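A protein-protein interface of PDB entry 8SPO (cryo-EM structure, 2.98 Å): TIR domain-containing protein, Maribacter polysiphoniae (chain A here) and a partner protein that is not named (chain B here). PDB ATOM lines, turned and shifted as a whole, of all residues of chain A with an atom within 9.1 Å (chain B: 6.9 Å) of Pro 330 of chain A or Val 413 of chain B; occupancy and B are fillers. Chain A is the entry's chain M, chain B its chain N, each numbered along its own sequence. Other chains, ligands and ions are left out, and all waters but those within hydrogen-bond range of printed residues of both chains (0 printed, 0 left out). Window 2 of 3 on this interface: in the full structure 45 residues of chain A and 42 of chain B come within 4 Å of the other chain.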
ATOM      1  N   TRP A 174     -14.116  -3.263 -13.491  1.00  0.00           N
ATOM      2  CA  TRP A 174     -13.067  -4.070 -14.100  1.00  0.00           C
ATOM      3  C   TRP A 174     -12.072  -3.154 -14.800  1.00  0.00           C
ATOM      4  O   TRP A 174     -12.458  -2.366 -15.671  1.00  0.00           O
ATOM      5  CB  TRP A 174     -13.654  -5.066 -15.098  1.00  0.00           C
ATOM      6  CG  TRP A 174     -14.239  -6.298 -14.479  1.00  0.00           C
ATOM      7  CD1 TRP A 174     -14.296  -6.605 -13.155  1.00  0.00           C
ATOM      8  CD2 TRP A 174     -14.848  -7.395 -15.170  1.00  0.00           C
ATOM      9  NE1 TRP A 174     -14.904  -7.821 -12.975  1.00  0.00           N
ATOM     10  CE2 TRP A 174     -15.250  -8.327 -14.199  1.00  0.00           C
ATOM     11  CE3 TRP A 174     -15.093  -7.675 -16.516  1.00  0.00           C
ATOM     12  CZ2 TRP A 174     -15.884  -9.521 -14.527  1.00  0.00           C
ATOM     13  CZ3 TRP A 174     -15.722  -8.858 -16.841  1.00  0.00           C
ATOM     14  CH2 TRP A 174     -16.111  -9.767 -15.851  1.00  0.00           C
ATOM     15  N   LEU A 246      -0.171 -17.686 -22.088  1.00  0.00           N
ATOM     16  CA  LEU A 246      -1.473 -17.077 -21.861  1.00  0.00           C
ATOM     17  C   LEU A 246      -2.512 -17.528 -22.876  1.00  0.00           C
ATOM     18  O   LEU A 246      -3.711 -17.484 -22.577  1.00  0.00           O
ATOM     19  CB  LEU A 246      -1.363 -15.547 -21.902  1.00  0.00           C
ATOM     20  CG  LEU A 246      -0.921 -14.813 -20.633  1.00  0.00           C
ATOM     21  CD1 LEU A 246      -1.144 -13.321 -20.802  1.00  0.00           C
ATOM     22  CD2 LEU A 246      -1.650 -15.314 -19.395  1.00  0.00           C
ATOM     23  N   LYS A 261      -0.230 -20.317 -15.181  1.00  0.00           N
ATOM     24  CA  LYS A 261      -1.202 -19.238 -15.029  1.00  0.00           C
ATOM     25  C   LYS A 261      -1.335 -18.832 -13.567  1.00  0.00           C
ATOM     26  O   LYS A 261      -1.424 -17.640 -13.248  1.00  0.00           O
ATOM     27  CB  LYS A 261      -2.560 -19.672 -15.582  1.00  0.00           C
ATOM     28  CG  LYS A 261      -2.588 -19.900 -17.081  1.00  0.00           C
ATOM     29  CD  LYS A 261      -4.003 -19.788 -17.619  1.00  0.00           C
ATOM     30  CE  LYS A 261      -4.035 -19.804 -19.139  1.00  0.00           C
ATOM     31  NZ  LYS A 261      -3.038 -20.741 -19.717  1.00  0.00           N
ATOM     32  N   LYS A 327      -7.388 -11.376 -12.339  1.00  0.00           N
ATOM     33  CA  LYS A 327      -7.900 -12.621 -12.888  1.00  0.00           C
ATOM     34  C   LYS A 327      -7.515 -12.725 -14.356  1.00  0.00           C
ATOM     35  O   LYS A 327      -7.261 -11.717 -15.020  1.00  0.00           O
ATOM     36  CB  LYS A 327      -9.424 -12.709 -12.749  1.00  0.00           C
ATOM     37  CG  LYS A 327      -9.927 -12.609 -11.321  1.00  0.00           C
ATOM     38  CD  LYS A 327      -9.359 -13.720 -10.455  1.00  0.00           C
ATOM     39  CE  LYS A 327     -10.352 -14.176  -9.401  1.00  0.00           C
ATOM     40  NZ  LYS A 327     -10.429 -13.230  -8.256  1.00  0.00           N
ATOM     41  N   LEU A 328      -7.466 -13.958 -14.855  1.00  0.00           N
ATOM     42  CA  LEU A 328      -7.167 -14.218 -16.256  1.00  0.00           C
ATOM     43  C   LEU A 328      -8.379 -14.694 -17.041  1.00  0.00           C
ATOM     44  O   LEU A 328      -8.262 -14.926 -18.249  1.00  0.00           O
ATOM     45  CB  LEU A 328      -6.041 -15.253 -16.372  1.00  0.00           C
ATOM     46  CG  LEU A 328      -4.650 -14.794 -15.925  1.00  0.00           C
ATOM     47  CD1 LEU A 328      -3.653 -15.924 -16.074  1.00  0.00           C
ATOM     48  CD2 LEU A 328      -4.191 -13.578 -16.712  1.00  0.00           C
ATOM     49  N   TYR A 329      -9.535 -14.843 -16.396  1.00  0.00           N
ATOM     50  CA  TYR A 329     -10.763 -15.241 -17.061  1.00  0.00           C
ATOM     51  C   TYR A 329     -11.856 -14.211 -16.795  1.00  0.00           C
ATOM     52  O   TYR A 329     -11.986 -13.732 -15.664  1.00  0.00           O
ATOM     53  CB  TYR A 329     -11.231 -16.624 -16.575  1.00  0.00           C
ATOM     54  CG  TYR A 329     -12.630 -16.997 -17.021  1.00  0.00           C
ATOM     55  CD1 TYR A 329     -12.842 -17.662 -18.222  1.00  0.00           C
ATOM     56  CD2 TYR A 329     -13.736 -16.688 -16.243  1.00  0.00           C
ATOM     57  CE1 TYR A 329     -14.115 -18.003 -18.636  1.00  0.00           C
ATOM     58  CE2 TYR A 329     -15.012 -17.025 -16.648  1.00  0.00           C
ATOM     59  CZ  TYR A 329     -15.195 -17.684 -17.843  1.00  0.00           C
ATOM     60  OH  TYR A 329     -16.466 -18.019 -18.249  1.00  0.00           O
ATOM     61  N   PRO A 330     -12.655 -13.841 -17.809  1.00  0.00           N
ATOM     62  CA  PRO A 330     -12.605 -14.265 -19.220  1.00  0.00           C
ATOM     63  C   PRO A 330     -11.394 -13.686 -19.942  1.00  0.00           C
ATOM     64  O   PRO A 330     -10.819 -14.326 -20.816  1.00  0.00           O
ATOM     65  CB  PRO A 330     -13.929 -13.733 -19.797  1.00  0.00           C
ATOM     66  CG  PRO A 330     -14.789 -13.400 -18.607  1.00  0.00           C
ATOM     67  CD  PRO A 330     -13.818 -12.980 -17.554  1.00  0.00           C
ATOM     68  N   PHE A 331     -10.989 -12.476 -19.588  1.00  0.00           N
ATOM     69  CA  PHE A 331      -9.811 -11.824 -20.136  1.00  0.00           C
ATOM     70  C   PHE A 331      -9.026 -11.182 -19.006  1.00  0.00           C
ATOM     71  O   PHE A 331      -9.578 -10.906 -17.935  1.00  0.00           O
ATOM     72  CB  PHE A 331     -10.193 -10.766 -21.183  1.00  0.00           C
ATOM     73  CG  PHE A 331     -11.217  -9.775 -20.707  1.00  0.00           C
ATOM     74  CD1 PHE A 331     -12.562 -10.106 -20.674  1.00  0.00           C
ATOM     75  CD2 PHE A 331     -10.839  -8.507 -20.307  1.00  0.00           C
ATOM     76  CE1 PHE A 331     -13.505  -9.195 -20.243  1.00  0.00           C
ATOM     77  CE2 PHE A 331     -11.779  -7.592 -19.881  1.00  0.00           C
ATOM     78  CZ  PHE A 331     -13.112  -7.939 -19.845  1.00  0.00           C
ATOM     79  N   PRO A 332      -7.724 -10.943 -19.204  1.00  0.00           N
ATOM     80  CA  PRO A 332      -6.926 -10.322 -18.138  1.00  0.00           C
ATOM     81  C   PRO A 332      -7.524  -9.017 -17.643  1.00  0.00           C
ATOM     82  O   PRO A 332      -7.596  -8.034 -18.384  1.00  0.00           O
ATOM     83  CB  PRO A 332      -5.568 -10.100 -18.810  1.00  0.00           C
ATOM     84  CG  PRO A 332      -5.485 -11.173 -19.825  1.00  0.00           C
ATOM     85  CD  PRO A 332      -6.886 -11.353 -20.343  1.00  0.00           C
ATOM     86  N   VAL A 333      -7.948  -9.001 -16.383  1.00  0.00           N
ATOM     87  CA  VAL A 333      -8.587  -7.854 -15.765  1.00  0.00           C
ATOM     88  C   VAL A 333      -7.937  -7.607 -14.411  1.00  0.00           C
ATOM     89  O   VAL A 333      -6.991  -8.289 -14.019  1.00  0.00           O
ATOM     90  CB  VAL A 333     -10.110  -8.050 -15.608  1.00  0.00           C
ATOM     91  CG1 VAL A 333     -10.783  -8.045 -16.958  1.00  0.00           C
ATOM     92  CG2 VAL A 333     -10.409  -9.343 -14.866  1.00  0.00           C
ATOM     93  N   MET A 335      -9.911  -6.744 -10.859  1.00  0.00           N
ATOM     94  CA  MET A 335     -11.188  -6.456 -10.223  1.00  0.00           C
ATOM     95  C   MET A 335     -10.995  -5.552  -9.013  1.00  0.00           C
ATOM     96  O   MET A 335     -10.042  -5.713  -8.246  1.00  0.00           O
ATOM     97  CB  MET A 335     -11.869  -7.758  -9.806  1.00  0.00           C
ATOM     98  CG  MET A 335     -12.212  -8.663 -10.977  1.00  0.00           C
ATOM     99  SD  MET A 335     -13.094 -10.159 -10.494  1.00  0.00           S
ATOM    100  CE  MET A 335     -13.369 -10.913 -12.094  1.00  0.00           C
ATOM    101  N   PHE A 409     -19.903  -1.401 -20.844  1.00  0.00           N
ATOM    102  CA  PHE A 409     -20.938  -2.299 -21.329  1.00  0.00           C
ATOM    103  C   PHE A 409     -22.046  -1.477 -21.965  1.00  0.00           C
ATOM    104  O   PHE A 409     -22.275  -0.324 -21.593  1.00  0.00           O
ATOM    105  CB  PHE A 409     -21.504  -3.168 -20.198  1.00  0.00           C
ATOM    106  CG  PHE A 409     -20.540  -4.199 -19.688  1.00  0.00           C
ATOM    107  CD1 PHE A 409     -19.496  -3.837 -18.854  1.00  0.00           C
ATOM    108  CD2 PHE A 409     -20.678  -5.529 -20.037  1.00  0.00           C
ATOM    109  CE1 PHE A 409     -18.606  -4.780 -18.388  1.00  0.00           C
ATOM    110  CE2 PHE A 409     -19.792  -6.476 -19.572  1.00  0.00           C
ATOM    111  CZ  PHE A 409     -18.756  -6.102 -18.744  1.00  0.00           C
ATOM    112  N   LYS B 392     -18.701 -13.690  -7.097  1.00  0.00           N
ATOM    113  CA  LYS B 392     -18.024 -13.207  -8.293  1.00  0.00           C
ATOM    114  C   LYS B 392     -18.159 -11.690  -8.377  1.00  0.00           C
ATOM    115  O   LYS B 392     -19.271 -11.184  -8.574  1.00  0.00           O
ATOM    116  CB  LYS B 392     -18.601 -13.870  -9.544  1.00  0.00           C
ATOM    117  CG  LYS B 392     -17.884 -13.505 -10.838  1.00  0.00           C
ATOM    118  CD  LYS B 392     -16.420 -13.933 -10.850  1.00  0.00           C
ATOM    119  CE  LYS B 392     -16.255 -15.446 -10.858  1.00  0.00           C
ATOM    120  NZ  LYS B 392     -16.634 -16.053 -12.161  1.00  0.00           N
ATOM    121  N   LEU B 394     -18.557  -8.460  -9.991  1.00  0.00           N
ATOM    122  CA  LEU B 394     -18.814  -7.730 -11.230  1.00  0.00           C
ATOM    123  C   LEU B 394     -20.027  -6.852 -10.992  1.00  0.00           C
ATOM    124  O   LEU B 394     -21.103  -7.363 -10.668  1.00  0.00           O
ATOM    125  CB  LEU B 394     -19.047  -8.671 -12.410  1.00  0.00           C
ATOM    126  CG  LEU B 394     -19.632  -8.015 -13.671  1.00  0.00           C
ATOM    127  CD1 LEU B 394     -18.656  -7.012 -14.262  1.00  0.00           C
ATOM    128  CD2 LEU B 394     -19.999  -9.060 -14.706  1.00  0.00           C
ATOM    129  N   TYR B 411     -25.164 -10.494 -19.270  1.00  0.00           N
ATOM    130  CA  TYR B 411     -23.973 -10.495 -20.107  1.00  0.00           C
ATOM    131  C   TYR B 411     -23.569 -11.942 -20.367  1.00  0.00           C
ATOM    132  O   TYR B 411     -23.311 -12.695 -19.423  1.00  0.00           O
ATOM    133  CB  TYR B 411     -22.837  -9.725 -19.437  1.00  0.00           C
ATOM    134  CG  TYR B 411     -21.476  -9.963 -20.050  1.00  0.00           C
ATOM    135  CD1 TYR B 411     -21.303  -9.958 -21.426  1.00  0.00           C
ATOM    136  CD2 TYR B 411     -20.364 -10.188 -19.253  1.00  0.00           C
ATOM    137  CE1 TYR B 411     -20.064 -10.178 -21.988  1.00  0.00           C
ATOM    138  CE2 TYR B 411     -19.122 -10.405 -19.807  1.00  0.00           C
ATOM    139  CZ  TYR B 411     -18.976 -10.401 -21.175  1.00  0.00           C
ATOM    140  OH  TYR B 411     -17.739 -10.619 -21.733  1.00  0.00           O
ATOM    141  N   VAL B 412     -23.514 -12.325 -21.638  1.00  0.00           N
ATOM    142  CA  VAL B 412     -23.237 -13.699 -22.041  1.00  0.00           C
ATOM    143  C   VAL B 412     -21.748 -13.794 -22.352  1.00  0.00           C
ATOM    144  O   VAL B 412     -21.301 -13.423 -23.441  1.00  0.00           O
ATOM    145  CB  VAL B 412     -24.094 -14.121 -23.235  1.00  0.00           C
ATOM    146  CG1 VAL B 412     -23.622 -15.455 -23.779  1.00  0.00           C
ATOM    147  CG2 VAL B 412     -25.556 -14.198 -22.836  1.00  0.00           C
ATOM    148  N   VAL B 413     -20.975 -14.310 -21.395  1.00  0.00           N
ATOM    149  CA  VAL B 413     -19.532 -14.406 -21.580  1.00  0.00           C
ATOM    150  C   VAL B 413     -19.199 -15.365 -22.714  1.00  0.00           C
ATOM    151  O   VAL B 413     -18.273 -15.122 -23.496  1.00  0.00           O
ATOM    152  CB  VAL B 413     -18.857 -14.839 -20.267  1.00  0.00           C
ATOM    153  CG1 VAL B 413     -17.438 -15.323 -20.535  1.00  0.00           C
ATOM    154  CG2 VAL B 413     -18.854 -13.695 -19.272  1.00  0.00           C
ATOM    155  N   ASN B 414     -19.937 -16.463 -22.818  1.00  0.00           N
ATOM    156  CA  ASN B 414     -19.603 -17.534 -23.743  1.00  0.00           C
ATOM    157  C   ASN B 414     -20.875 -18.310 -24.058  1.00  0.00           C
ATOM    158  O   ASN B 414     -21.986 -17.877 -23.734  1.00  0.00           O
ATOM    159  CB  ASN B 414     -18.520 -18.435 -23.137  1.00  0.00           C
ATOM    160  CG  ASN B 414     -17.572 -18.986 -24.170  1.00  0.00           C
ATOM    161  OD1 ASN B 414     -17.833 -18.914 -25.369  1.00  0.00           O
ATOM    162  ND2 ASN B 414     -16.462 -19.545 -23.710  1.00  0.00           N
ATOM    163  N   GLU B 415     -20.712 -19.465 -24.698  1.00  0.00           N
ATOM    164  CA  GLU B 415     -21.823 -20.388 -24.871  1.00  0.00           C
ATOM    165  C   GLU B 415     -22.053 -21.243 -23.631  1.00  0.00           C
ATOM    166  O   GLU B 415     -23.074 -21.933 -23.551  1.00  0.00           O
ATOM    167  CB  GLU B 415     -21.566 -21.280 -26.089  1.00  0.00           C
ATOM    168  CG  GLU B 415     -22.594 -22.383 -26.306  1.00  0.00           C
ATOM    169  CD  GLU B 415     -24.020 -21.866 -26.317  1.00  0.00           C
ATOM    170  OE1 GLU B 415     -24.231 -20.711 -26.740  1.00  0.00           O
ATOM    171  OE2 GLU B 415     -24.926 -22.617 -25.901  1.00  0.00           O
ATOM    172  N   ARG B 416     -21.139 -21.197 -22.658  1.00  0.00           N
ATOM    173  CA  ARG B 416     -21.235 -22.004 -21.447  1.00  0.00           C
ATOM    174  C   ARG B 416     -21.117 -21.163 -20.179  1.00  0.00           C
ATOM    175  O   ARG B 416     -20.820 -21.705 -19.111  1.00  0.00           O
ATOM    176  CB  ARG B 416     -20.163 -23.093 -21.457  1.00  0.00           C
ATOM    177  CG  ARG B 416     -20.426 -24.192 -22.465  1.00  0.00           C
ATOM    178  CD  ARG B 416     -19.334 -25.245 -22.443  1.00  0.00           C
ATOM    179  NE  ARG B 416     -19.639 -26.330 -21.520  1.00  0.00           N
ATOM    180  CZ  ARG B 416     -20.582 -27.241 -21.720  1.00  0.00           C
ATOM    181  NH1 ARG B 416     -21.334 -27.231 -22.808  1.00  0.00           N
ATOM    182  NH2 ARG B 416     -20.774 -28.185 -20.804  1.00  0.00           N
ATOM    183  N   SER B 417     -21.340 -19.855 -20.271  1.00  0.00           N
ATOM    184  CA  SER B 417     -21.324 -19.000 -19.092  1.00  0.00           C
ATOM    185  C   SER B 417     -22.106 -17.735 -19.401  1.00  0.00           C
ATOM    186  O   SER B 417     -22.337 -17.395 -20.564  1.00  0.00           O
ATOM    187  CB  SER B 417     -19.895 -18.654 -18.662  1.00  0.00           C
ATOM    188  OG  SER B 417     -19.112 -19.820 -18.498  1.00  0.00           O
ATOM    189  N   ALA B 418     -22.513 -17.045 -18.341  1.00  0.00           N
ATOM    190  CA  ALA B 418     -23.227 -15.785 -18.476  1.00  0.00           C
ATOM    191  C   ALA B 418     -23.463 -15.202 -17.091  1.00  0.00           C
ATOM    192  O   ALA B 418     -23.481 -15.928 -16.095  1.00  0.00           O
ATOM    193  CB  ALA B 418     -24.563 -15.973 -19.205  1.00  0.00           C
ATOM    194  N   PHE B 419     -23.642 -13.888 -17.047  1.00  0.00           N
ATOM    195  CA  PHE B 419     -24.020 -13.172 -15.835  1.00  0.00           C
ATOM    196  C   PHE B 419     -25.482 -12.771 -15.967  1.00  0.00           C
ATOM    197  O   PHE B 419     -25.869 -12.162 -16.967  1.00  0.00           O
ATOM    198  CB  PHE B 419     -23.145 -11.935 -15.629  1.00  0.00           C
ATOM    199  CG  PHE B 419     -21.799 -12.228 -15.039  1.00  0.00           C
ATOM    200  CD1 PHE B 419     -20.719 -12.520 -15.852  1.00  0.00           C
ATOM    201  CD2 PHE B 419     -21.612 -12.194 -13.671  1.00  0.00           C
ATOM    202  CE1 PHE B 419     -19.479 -12.780 -15.306  1.00  0.00           C
ATOM    203  CE2 PHE B 419     -20.375 -12.453 -13.123  1.00  0.00           C
ATOM    204  CZ  PHE B 419     -19.308 -12.746 -13.940  1.00  0.00           C
ATOM    205  N   PHE B 442     -23.834 -15.765 -11.300  1.00  0.00           N
ATOM    206  CA  PHE B 442     -22.960 -16.362 -12.300  1.00  0.00           C
ATOM    207  C   PHE B 442     -23.447 -17.777 -12.590  1.00  0.00           C
ATOM    208  O   PHE B 442     -23.421 -18.639 -11.705  1.00  0.00           O
ATOM    209  CB  PHE B 442     -21.511 -16.367 -11.813  1.00  0.00           C
ATOM    210  CG  PHE B 442     -20.511 -16.657 -12.893  1.00  0.00           C
ATOM    211  CD1 PHE B 442     -20.493 -15.911 -14.055  1.00  0.00           C
ATOM    212  CD2 PHE B 442     -19.592 -17.677 -12.749  1.00  0.00           C
ATOM    213  CE1 PHE B 442     -19.578 -16.174 -15.052  1.00  0.00           C
ATOM    214  CE2 PHE B 442     -18.675 -17.946 -13.742  1.00  0.00           C
ATOM    215  CZ  PHE B 442     -18.669 -17.194 -14.896  1.00  0.00           C
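OH of Tyr 329 of chain A sits at hydrogen-bond distance from OG of Ser 417 of chain B.
Printed residues of chain B within 4 Å of Trp 174 of chain A: Leu 394 (3.7 Å). Lys 327 of chain A touches none of the printed residues of chain B. Of the printed residues of chain B, Tyr 329 of chain A touches Val 413 and Ser 417. Pro 330 of chain A touches just one residue of chain B: Val 413. Of the printed residues of chain B, Phe 409 of chain A touches Tyr 411 (3.8 Å). No residue of chain A comes within 4 Å of Val 412 of chain B. Of chain A, only Tyr 329 (3.7 Å) and Pro 330 (3.8 Å) come within 4 Å of Val 413 of chain B. No residue of chain A comes within 4 Å of Asn 414 of chain B. Of the printed residues of chain A, Ser 417 of chain B touches Tyr 329 (3.2 Å). Ala 418 of chain B touches none of the printed residues of chain A. The nearest residue of chain B that does not touch Pro 330 of chain A is Tyr 411 of chain B (5.1 Å). The nearest printed residue of chain A that does not touch Tyr 411 of chain B is Phe 331 of chain A (4.7 Å).
The backbone carbonyl oxygen (O) of Tyr 411 of chain B is in hydrogen-bond range of the backbone NH (N) of Phe 419 of chain B (2.7 Å).
Hydrophobic or aromatic side chains of chain A that line the printed part of chain B: Trp 174, Tyr 329, Pro 330 and Phe 409. Of the 12 printed residues of chain B, 4 touch a printed residue of chain A. Hydrophobic or aromatic side chains of chain B within 4 Å of the printed part of chain A: Leu 394, Tyr 411 and Val 413. Along chain B the printed residues that touch a printed residue of chain A span positions 394 to 417. Among the printed residues, no Asp or Glu carboxylate lies within 4 Å of a Lys or Arg side-chain nitrogen of the other chain.
Among the printed residues, pairs that only touch across the chains: Trp 174 of chain A with Leu 394 of chain B, Tyr 329 of chain A with Val 413 of chain B, Phe 409 of chain A with Tyr 411 of chain B and Pro 330 of chain A with Val 413 of chain B.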
